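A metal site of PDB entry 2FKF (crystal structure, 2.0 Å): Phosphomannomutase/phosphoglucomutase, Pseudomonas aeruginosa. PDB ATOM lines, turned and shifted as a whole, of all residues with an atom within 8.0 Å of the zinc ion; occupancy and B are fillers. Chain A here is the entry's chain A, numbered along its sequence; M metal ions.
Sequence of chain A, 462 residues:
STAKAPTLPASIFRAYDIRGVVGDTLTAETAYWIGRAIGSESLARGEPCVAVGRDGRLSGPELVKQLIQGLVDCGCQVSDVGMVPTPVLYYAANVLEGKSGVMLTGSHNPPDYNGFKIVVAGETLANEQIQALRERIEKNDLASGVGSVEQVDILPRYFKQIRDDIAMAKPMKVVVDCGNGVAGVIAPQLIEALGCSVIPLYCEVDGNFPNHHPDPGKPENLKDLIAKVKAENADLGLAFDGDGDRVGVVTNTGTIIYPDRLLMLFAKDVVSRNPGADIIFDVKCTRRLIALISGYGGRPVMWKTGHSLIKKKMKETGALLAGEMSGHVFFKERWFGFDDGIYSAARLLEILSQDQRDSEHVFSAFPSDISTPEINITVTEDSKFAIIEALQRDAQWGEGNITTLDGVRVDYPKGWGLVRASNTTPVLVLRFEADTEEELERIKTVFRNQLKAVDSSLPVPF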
ATOM      1  N   ARG A  19     -11.119   4.924  10.531  1.00  0.00           N
ATOM      2  CA  ARG A  19     -11.157   4.270   9.228  1.00  0.00           C
ATOM      3  C   ARG A  19     -10.519   2.888   9.347  1.00  0.00           C
ATOM      4  O   ARG A  19      -9.423   2.764   9.913  1.00  0.00           O
ATOM      5  CB  ARG A  19     -10.375   5.091   8.197  1.00  0.00           C
ATOM      6  CG  ARG A  19     -10.538   4.627   6.744  1.00  0.00           C
ATOM      7  CD  ARG A  19     -11.897   5.009   6.166  1.00  0.00           C
ATOM      8  NE  ARG A  19     -12.122   6.456   6.219  1.00  0.00           N
ATOM      9  CZ  ARG A  19     -11.661   7.341   5.325  1.00  0.00           C
ATOM     10  NH1 ARG A  19     -10.933   6.941   4.293  1.00  0.00           N
ATOM     11  NH2 ARG A  19     -11.912   8.622   5.487  1.00  0.00           N
ATOM     12  N   THR A  86     -22.132  12.845   3.454  1.00  0.00           N
ATOM     13  CA  THR A  86     -21.494  13.378   4.649  1.00  0.00           C
ATOM     14  C   THR A  86     -21.936  14.799   4.989  1.00  0.00           C
ATOM     15  O   THR A  86     -22.267  15.070   6.136  1.00  0.00           O
ATOM     16  CB  THR A  86     -19.979  13.305   4.502  1.00  0.00           C
ATOM     17  OG1 THR A  86     -19.573  11.930   4.535  1.00  0.00           O
ATOM     18  CG2 THR A  86     -19.281  14.062   5.617  1.00  0.00           C
ATOM     19  N   PRO A  87     -21.914  15.722   4.009  1.00  0.00           N
ATOM     20  CA  PRO A  87     -22.396  17.073   4.354  1.00  0.00           C
ATOM     21  C   PRO A  87     -23.828  17.169   4.842  1.00  0.00           C
ATOM     22  O   PRO A  87     -24.153  18.122   5.539  1.00  0.00           O
ATOM     23  CB  PRO A  87     -22.255  17.856   3.041  1.00  0.00           C
ATOM     24  CG  PRO A  87     -22.112  16.847   1.974  1.00  0.00           C
ATOM     25  CD  PRO A  87     -21.437  15.664   2.615  1.00  0.00           C
ATOM     26  N   TYR A  90     -23.603  16.465   8.462  1.00  0.00           N
ATOM     27  CA  TYR A  90     -23.120  17.698   9.096  1.00  0.00           C
ATOM     28  C   TYR A  90     -24.253  18.723   9.193  1.00  0.00           C
ATOM     29  O   TYR A  90     -24.396  19.431  10.196  1.00  0.00           O
ATOM     30  CB  TYR A  90     -21.975  18.327   8.291  1.00  0.00           C
ATOM     31  CG  TYR A  90     -20.676  17.538   8.244  1.00  0.00           C
ATOM     32  CD1 TYR A  90     -20.368  16.573   9.191  1.00  0.00           C
ATOM     33  CD2 TYR A  90     -19.747  17.803   7.246  1.00  0.00           C
ATOM     34  CE1 TYR A  90     -19.153  15.872   9.146  1.00  0.00           C
ATOM     35  CE2 TYR A  90     -18.528  17.114   7.183  1.00  0.00           C
ATOM     36  CZ  TYR A  90     -18.241  16.148   8.135  1.00  0.00           C
ATOM     37  OH  TYR A  90     -17.047  15.466   8.088  1.00  0.00           O
ATOM     38  N   THR A 105     -18.809   6.350   7.283  1.00  0.00           N
ATOM     39  CA  THR A 105     -18.327   6.378   5.897  1.00  0.00           C
ATOM     40  C   THR A 105     -16.865   5.946   5.743  1.00  0.00           C
ATOM     41  O   THR A 105     -16.046   6.134   6.641  1.00  0.00           O
ATOM     42  CB  THR A 105     -18.524   7.767   5.277  1.00  0.00           C
ATOM     43  OG1 THR A 105     -18.110   7.748   3.900  1.00  0.00           O
ATOM     44  CG2 THR A 105     -17.719   8.824   6.023  1.00  0.00           C
ATOM     45  N   GLY A 106     -16.577   5.358   4.589  1.00  0.00           N
ATOM     46  CA  GLY A 106     -15.204   5.068   4.167  1.00  0.00           C
ATOM     47  C   GLY A 106     -14.724   5.986   3.053  1.00  0.00           C
ATOM     48  O   GLY A 106     -13.743   5.682   2.372  1.00  0.00           O
ATOM     49  N   SEP A 107     -15.418   7.111   2.876  1.00  0.00           N
ATOM     50  CA  SEP A 107     -15.050   8.180   1.945  1.00  0.00           C
ATOM     51  CB  SEP A 107     -13.785   8.879   2.461  1.00  0.00           C
ATOM     52  OG  SEP A 107     -13.319   9.857   1.551  1.00  0.00           O
ATOM     53  C   SEP A 107     -14.924   7.685   0.485  1.00  0.00           C
ATOM     54  O   SEP A 107     -15.928   7.310  -0.141  1.00  0.00           O
ATOM     55  P   SEP A 107     -12.674  11.181   2.252  1.00  0.00           P
ATOM     56  O1P SEP A 107     -11.302  11.542   1.503  1.00  0.00           O
ATOM     57  O2P SEP A 107     -12.424  10.968   3.814  1.00  0.00           O
ATOM     58  O3P SEP A 107     -13.701  12.376   2.013  1.00  0.00           O
ATOM     59  N   HIS A 108     -13.700   7.657  -0.039  1.00  0.00           N
ATOM     60  CA  HIS A 108     -13.460   7.237  -1.424  1.00  0.00           C
ATOM     61  C   HIS A 108     -12.720   5.905  -1.513  1.00  0.00           C
ATOM     62  O   HIS A 108     -12.348   5.471  -2.599  1.00  0.00           O
ATOM     63  CB  HIS A 108     -12.667   8.324  -2.163  1.00  0.00           C
ATOM     64  CG  HIS A 108     -11.284   8.519  -1.624  1.00  0.00           C
ATOM     65  ND1 HIS A 108     -10.228   7.720  -1.984  1.00  0.00           N
ATOM     66  CD2 HIS A 108     -10.801   9.407  -0.721  1.00  0.00           C
ATOM     67  CE1 HIS A 108      -9.136   8.117  -1.341  1.00  0.00           C
ATOM     68  NE2 HIS A 108      -9.457   9.144  -0.572  1.00  0.00           N
ATOM     69  N   ASN A 109     -12.503   5.252  -0.382  1.00  0.00           N
ATOM     70  CA  ASN A 109     -11.735   3.996  -0.322  1.00  0.00           C
ATOM     71  C   ASN A 109     -12.462   2.832  -1.012  1.00  0.00           C
ATOM     72  O   ASN A 109     -13.640   2.961  -1.358  1.00  0.00           O
ATOM     73  CB  ASN A 109     -11.428   3.656   1.133  1.00  0.00           C
ATOM     74  CG  ASN A 109     -10.432   4.632   1.775  1.00  0.00           C
ATOM     75  OD1 ASN A 109     -10.295   4.660   3.006  1.00  0.00           O
ATOM     76  ND2 ASN A 109      -9.738   5.407   0.954  1.00  0.00           N
ATOM     77  N   LYS A 117     -16.768   9.718  10.766  1.00  0.00           N
ATOM     78  CA  LYS A 117     -16.432  11.132  10.925  1.00  0.00           C
ATOM     79  C   LYS A 117     -17.347  11.691  12.012  1.00  0.00           C
ATOM     80  O   LYS A 117     -18.563  11.470  11.973  1.00  0.00           O
ATOM     81  CB  LYS A 117     -16.582  11.880   9.604  1.00  0.00           C
ATOM     82  CG  LYS A 117     -15.761  11.243   8.496  1.00  0.00           C
ATOM     83  CD  LYS A 117     -15.740  12.094   7.252  1.00  0.00           C
ATOM     84  CE  LYS A 117     -14.973  11.390   6.126  1.00  0.00           C
ATOM     85  NZ  LYS A 117     -14.730  12.281   4.932  1.00  0.00           N
ATOM     86  N   PRO A 214     -14.729   6.328  -6.659  1.00  0.00           N
ATOM     87  CA  PRO A 214     -15.281   7.686  -6.511  1.00  0.00           C
ATOM     88  C   PRO A 214     -14.297   8.638  -5.800  1.00  0.00           C
ATOM     89  O   PRO A 214     -14.530   9.029  -4.645  1.00  0.00           O
ATOM     90  CB  PRO A 214     -16.544   7.445  -5.695  1.00  0.00           C
ATOM     91  CG  PRO A 214     -16.182   6.282  -4.828  1.00  0.00           C
ATOM     92  CD  PRO A 214     -15.217   5.424  -5.604  1.00  0.00           C
ATOM     93  N   PRO A 216     -12.417  11.965  -7.169  1.00  0.00           N
ATOM     94  CA  PRO A 216     -12.143  12.975  -8.210  1.00  0.00           C
ATOM     95  C   PRO A 216     -10.779  13.655  -8.132  1.00  0.00           C
ATOM     96  O   PRO A 216     -10.468  14.469  -9.005  1.00  0.00           O
ATOM     97  CB  PRO A 216     -13.256  14.012  -8.008  1.00  0.00           C
ATOM     98  CG  PRO A 216     -13.729  13.820  -6.615  1.00  0.00           C
ATOM     99  CD  PRO A 216     -13.504  12.389  -6.263  1.00  0.00           C
ATOM    100  N   PHE A 240     -18.108  13.929  -7.930  1.00  0.00           N
ATOM    101  CA  PHE A 240     -18.200  13.860  -6.479  1.00  0.00           C
ATOM    102  C   PHE A 240     -17.446  12.660  -5.976  1.00  0.00           C
ATOM    103  O   PHE A 240     -17.333  11.652  -6.681  1.00  0.00           O
ATOM    104  CB  PHE A 240     -19.676  13.811  -6.058  1.00  0.00           C
ATOM    105  CG  PHE A 240     -20.410  15.082  -6.383  1.00  0.00           C
ATOM    106  CD1 PHE A 240     -20.249  16.197  -5.593  1.00  0.00           C
ATOM    107  CD2 PHE A 240     -21.186  15.185  -7.515  1.00  0.00           C
ATOM    108  CE1 PHE A 240     -20.898  17.373  -5.914  1.00  0.00           C
ATOM    109  CE2 PHE A 240     -21.821  16.365  -7.835  1.00  0.00           C
ATOM    110  CZ  PHE A 240     -21.684  17.457  -7.034  1.00  0.00           C
ATOM    111  N   ASP A 241     -16.877  12.780  -4.769  1.00  0.00           N
ATOM    112  CA  ASP A 241     -16.269  11.629  -4.134  1.00  0.00           C
ATOM    113  C   ASP A 241     -17.370  10.795  -3.480  1.00  0.00           C
ATOM    114  O   ASP A 241     -18.543  11.216  -3.438  1.00  0.00           O
ATOM    115  CB  ASP A 241     -15.140  12.009  -3.169  1.00  0.00           C
ATOM    116  CG  ASP A 241     -15.626  12.441  -1.797  1.00  0.00           C
ATOM    117  OD1 ASP A 241     -16.739  13.001  -1.680  1.00  0.00           O
ATOM    118  OD2 ASP A 241     -14.848  12.261  -0.823  1.00  0.00           O
ATOM    119  N   GLY A 242     -16.984   9.625  -2.982  1.00  0.00           N
ATOM    120  CA  GLY A 242     -17.932   8.624  -2.495  1.00  0.00           C
ATOM    121  C   GLY A 242     -18.947   9.076  -1.463  1.00  0.00           C
ATOM    122  O   GLY A 242     -20.080   8.580  -1.462  1.00  0.00           O
ATOM    123  N   ASP A 243     -18.546   9.970  -0.578  1.00  0.00           N
ATOM    124  CA  ASP A 243     -19.423  10.453   0.469  1.00  0.00           C
ATOM    125  C   ASP A 243     -19.898  11.907   0.248  1.00  0.00           C
ATOM    126  O   ASP A 243     -20.660  12.428   1.052  1.00  0.00           O
ATOM    127  CB  ASP A 243     -18.782  10.251   1.856  1.00  0.00           C
ATOM    128  CG  ASP A 243     -17.492  11.040   2.040  1.00  0.00           C
ATOM    129  OD1 ASP A 243     -16.725  11.113   1.079  1.00  0.00           O
ATOM    130  OD2 ASP A 243     -17.259  11.566   3.148  1.00  0.00           O
ATOM    131  N   GLY A 244     -19.446  12.549  -0.828  1.00  0.00           N
ATOM    132  CA  GLY A 244     -19.985  13.855  -1.245  1.00  0.00           C
ATOM    133  C   GLY A 244     -19.467  15.109  -0.562  1.00  0.00           C
ATOM    134  O   GLY A 244     -20.025  16.192  -0.733  1.00  0.00           O
ATOM    135  N   ASP A 245     -18.406  14.984   0.221  1.00  0.00           N
ATOM    136  CA  ASP A 245     -17.794  16.183   0.826  1.00  0.00           C
ATOM    137  C   ASP A 245     -16.646  16.760  -0.011  1.00  0.00           C
ATOM    138  O   ASP A 245     -16.044  17.753   0.392  1.00  0.00           O
ATOM    139  CB  ASP A 245     -17.314  15.892   2.246  1.00  0.00           C
ATOM    140  CG  ASP A 245     -16.326  14.769   2.311  1.00  0.00           C
ATOM    141  OD1 ASP A 245     -15.999  14.180   1.240  1.00  0.00           O
ATOM    142  OD2 ASP A 245     -15.906  14.466   3.443  1.00  0.00           O
ATOM    143  N   ARG A 246     -16.346  16.125  -1.146  1.00  0.00           N
ATOM    144  CA  ARG A 246     -15.365  16.640  -2.109  1.00  0.00           C
ATOM    145  C   ARG A 246     -15.987  16.676  -3.511  1.00  0.00           C
ATOM    146  O   ARG A 246     -16.782  15.785  -3.864  1.00  0.00           O
ATOM    147  CB  ARG A 246     -14.121  15.756  -2.145  1.00  0.00           C
ATOM    148  CG  ARG A 246     -13.346  15.671  -0.845  1.00  0.00           C
ATOM    149  CD  ARG A 246     -11.973  15.020  -1.067  1.00  0.00           C
ATOM    150  NE  ARG A 246     -12.042  13.587  -1.292  1.00  0.00           N
ATOM    151  CZ  ARG A 246     -11.606  12.954  -2.382  1.00  0.00           C
ATOM    152  NH1 ARG A 246     -11.013  13.605  -3.390  1.00  0.00           N
ATOM    153  NH2 ARG A 246     -11.749  11.645  -2.467  1.00  0.00           N
ATOM    154  N   VAL A 247     -15.594  17.675  -4.294  1.00  0.00           N
ATOM    155  CA  VAL A 247     -16.066  17.826  -5.678  1.00  0.00           C
ATOM    156  C   VAL A 247     -14.885  18.144  -6.601  1.00  0.00           C
ATOM    157  O   VAL A 247     -13.987  18.899  -6.219  1.00  0.00           O
ATOM    158  CB  VAL A 247     -17.153  18.921  -5.813  1.00  0.00           C
ATOM    159  CG1 VAL A 247     -16.612  20.294  -5.440  1.00  0.00           C
ATOM    160  CG2 VAL A 247     -17.745  18.927  -7.212  1.00  0.00           C
ATOM    161  N   SER A 326      -7.147  18.721  -1.669  1.00  0.00           N
ATOM    162  CA  SER A 326      -7.859  17.447  -1.872  1.00  0.00           C
ATOM    163  C   SER A 326      -9.311  17.630  -2.299  1.00  0.00           C
ATOM    164  O   SER A 326      -9.997  16.640  -2.546  1.00  0.00           O
ATOM    165  CB  SER A 326      -7.751  16.554  -0.635  1.00  0.00           C
ATOM    166  OG  SER A 326      -6.415  16.133  -0.451  1.00  0.00           O
ATOM    167  N   HIS A 328     -11.861  19.520  -0.695  1.00  0.00           N
ATOM    168  CA  HIS A 328     -12.813  19.941   0.314  1.00  0.00           C
ATOM    169  C   HIS A 328     -12.941  21.478   0.289  1.00  0.00           C
ATOM    170  O   HIS A 328     -11.951  22.190   0.431  1.00  0.00           O
ATOM    171  CB  HIS A 328     -12.377  19.471   1.703  1.00  0.00           C
ATOM    172  CG  HIS A 328     -12.470  17.995   1.929  1.00  0.00           C
ATOM    173  ND1 HIS A 328     -11.409  17.140   1.740  1.00  0.00           N
ATOM    174  CD2 HIS A 328     -13.492  17.239   2.383  1.00  0.00           C
ATOM    175  CE1 HIS A 328     -11.786  15.900   2.046  1.00  0.00           C
ATOM    176  NE2 HIS A 328     -13.051  15.943   2.439  1.00  0.00           N
ATOM    177  N   ASP A 339     -17.385  21.304   5.134  1.00  0.00           N
ATOM    178  CA  ASP A 339     -17.063  20.907   3.754  1.00  0.00           C
ATOM    179  C   ASP A 339     -18.236  20.195   3.101  1.00  0.00           C
ATOM    180  O   ASP A 339     -18.893  19.362   3.712  1.00  0.00           O
ATOM    181  CB  ASP A 339     -15.796  20.053   3.684  1.00  0.00           C
ATOM    182  CG  ASP A 339     -15.674  19.052   4.816  1.00  0.00           C
ATOM    183  OD1 ASP A 339     -16.058  19.358   5.958  1.00  0.00           O
ATOM    184  OD2 ASP A 339     -15.146  17.961   4.568  1.00  0.00           O
HETATM  185 ZN    ZN M   1     -15.195  12.456   1.055  1.00  0.00          ZN
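NZ of Lys 117 lies within salt-bridge range of OD2 of Asp 245 (2.9 Å).
OD2 of Asp 243 is in salt-bridge range of NZ of Lys 117, at 3.2 Å.
The side-chain carboxylate of Asp 243 sits at hydrogen-bond distance from the side-chain hydroxyl of Thr 86, at 2.7 Å.
O2P of SEP 107 lies within salt-bridge range of NH2 of Arg 19 (2.9 Å).
The side-chain hydroxyl (OG1) of Thr 105 sits at hydrogen-bond distance from N of SEP 107, at 2.9 Å.
OD1 of Asp 241 sits at hydrogen-bond distance from N of Gly 244 (2.9 Å).
The backbone carbonyl oxygen of Arg 246 is in hydrogen-bond range of the backbone NH of Asp 241, 3.1 Å away.
The side-chain amino group of Lys 117 lies within salt-bridge range of O2P of SEP 107, at 2.9 Å.
The zinc ion is bound by O3P of SEP 107 (1.8 Å), OD1 of Asp 245 (1.9 Å), OD2 of Asp 241 (1.9 Å) and OD1 of Asp 243 (2.0 Å).
The zinc ion has four donor atoms within binding distance.
NZ of Lys 117 touches the zinc ion, at 3.9 Å.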
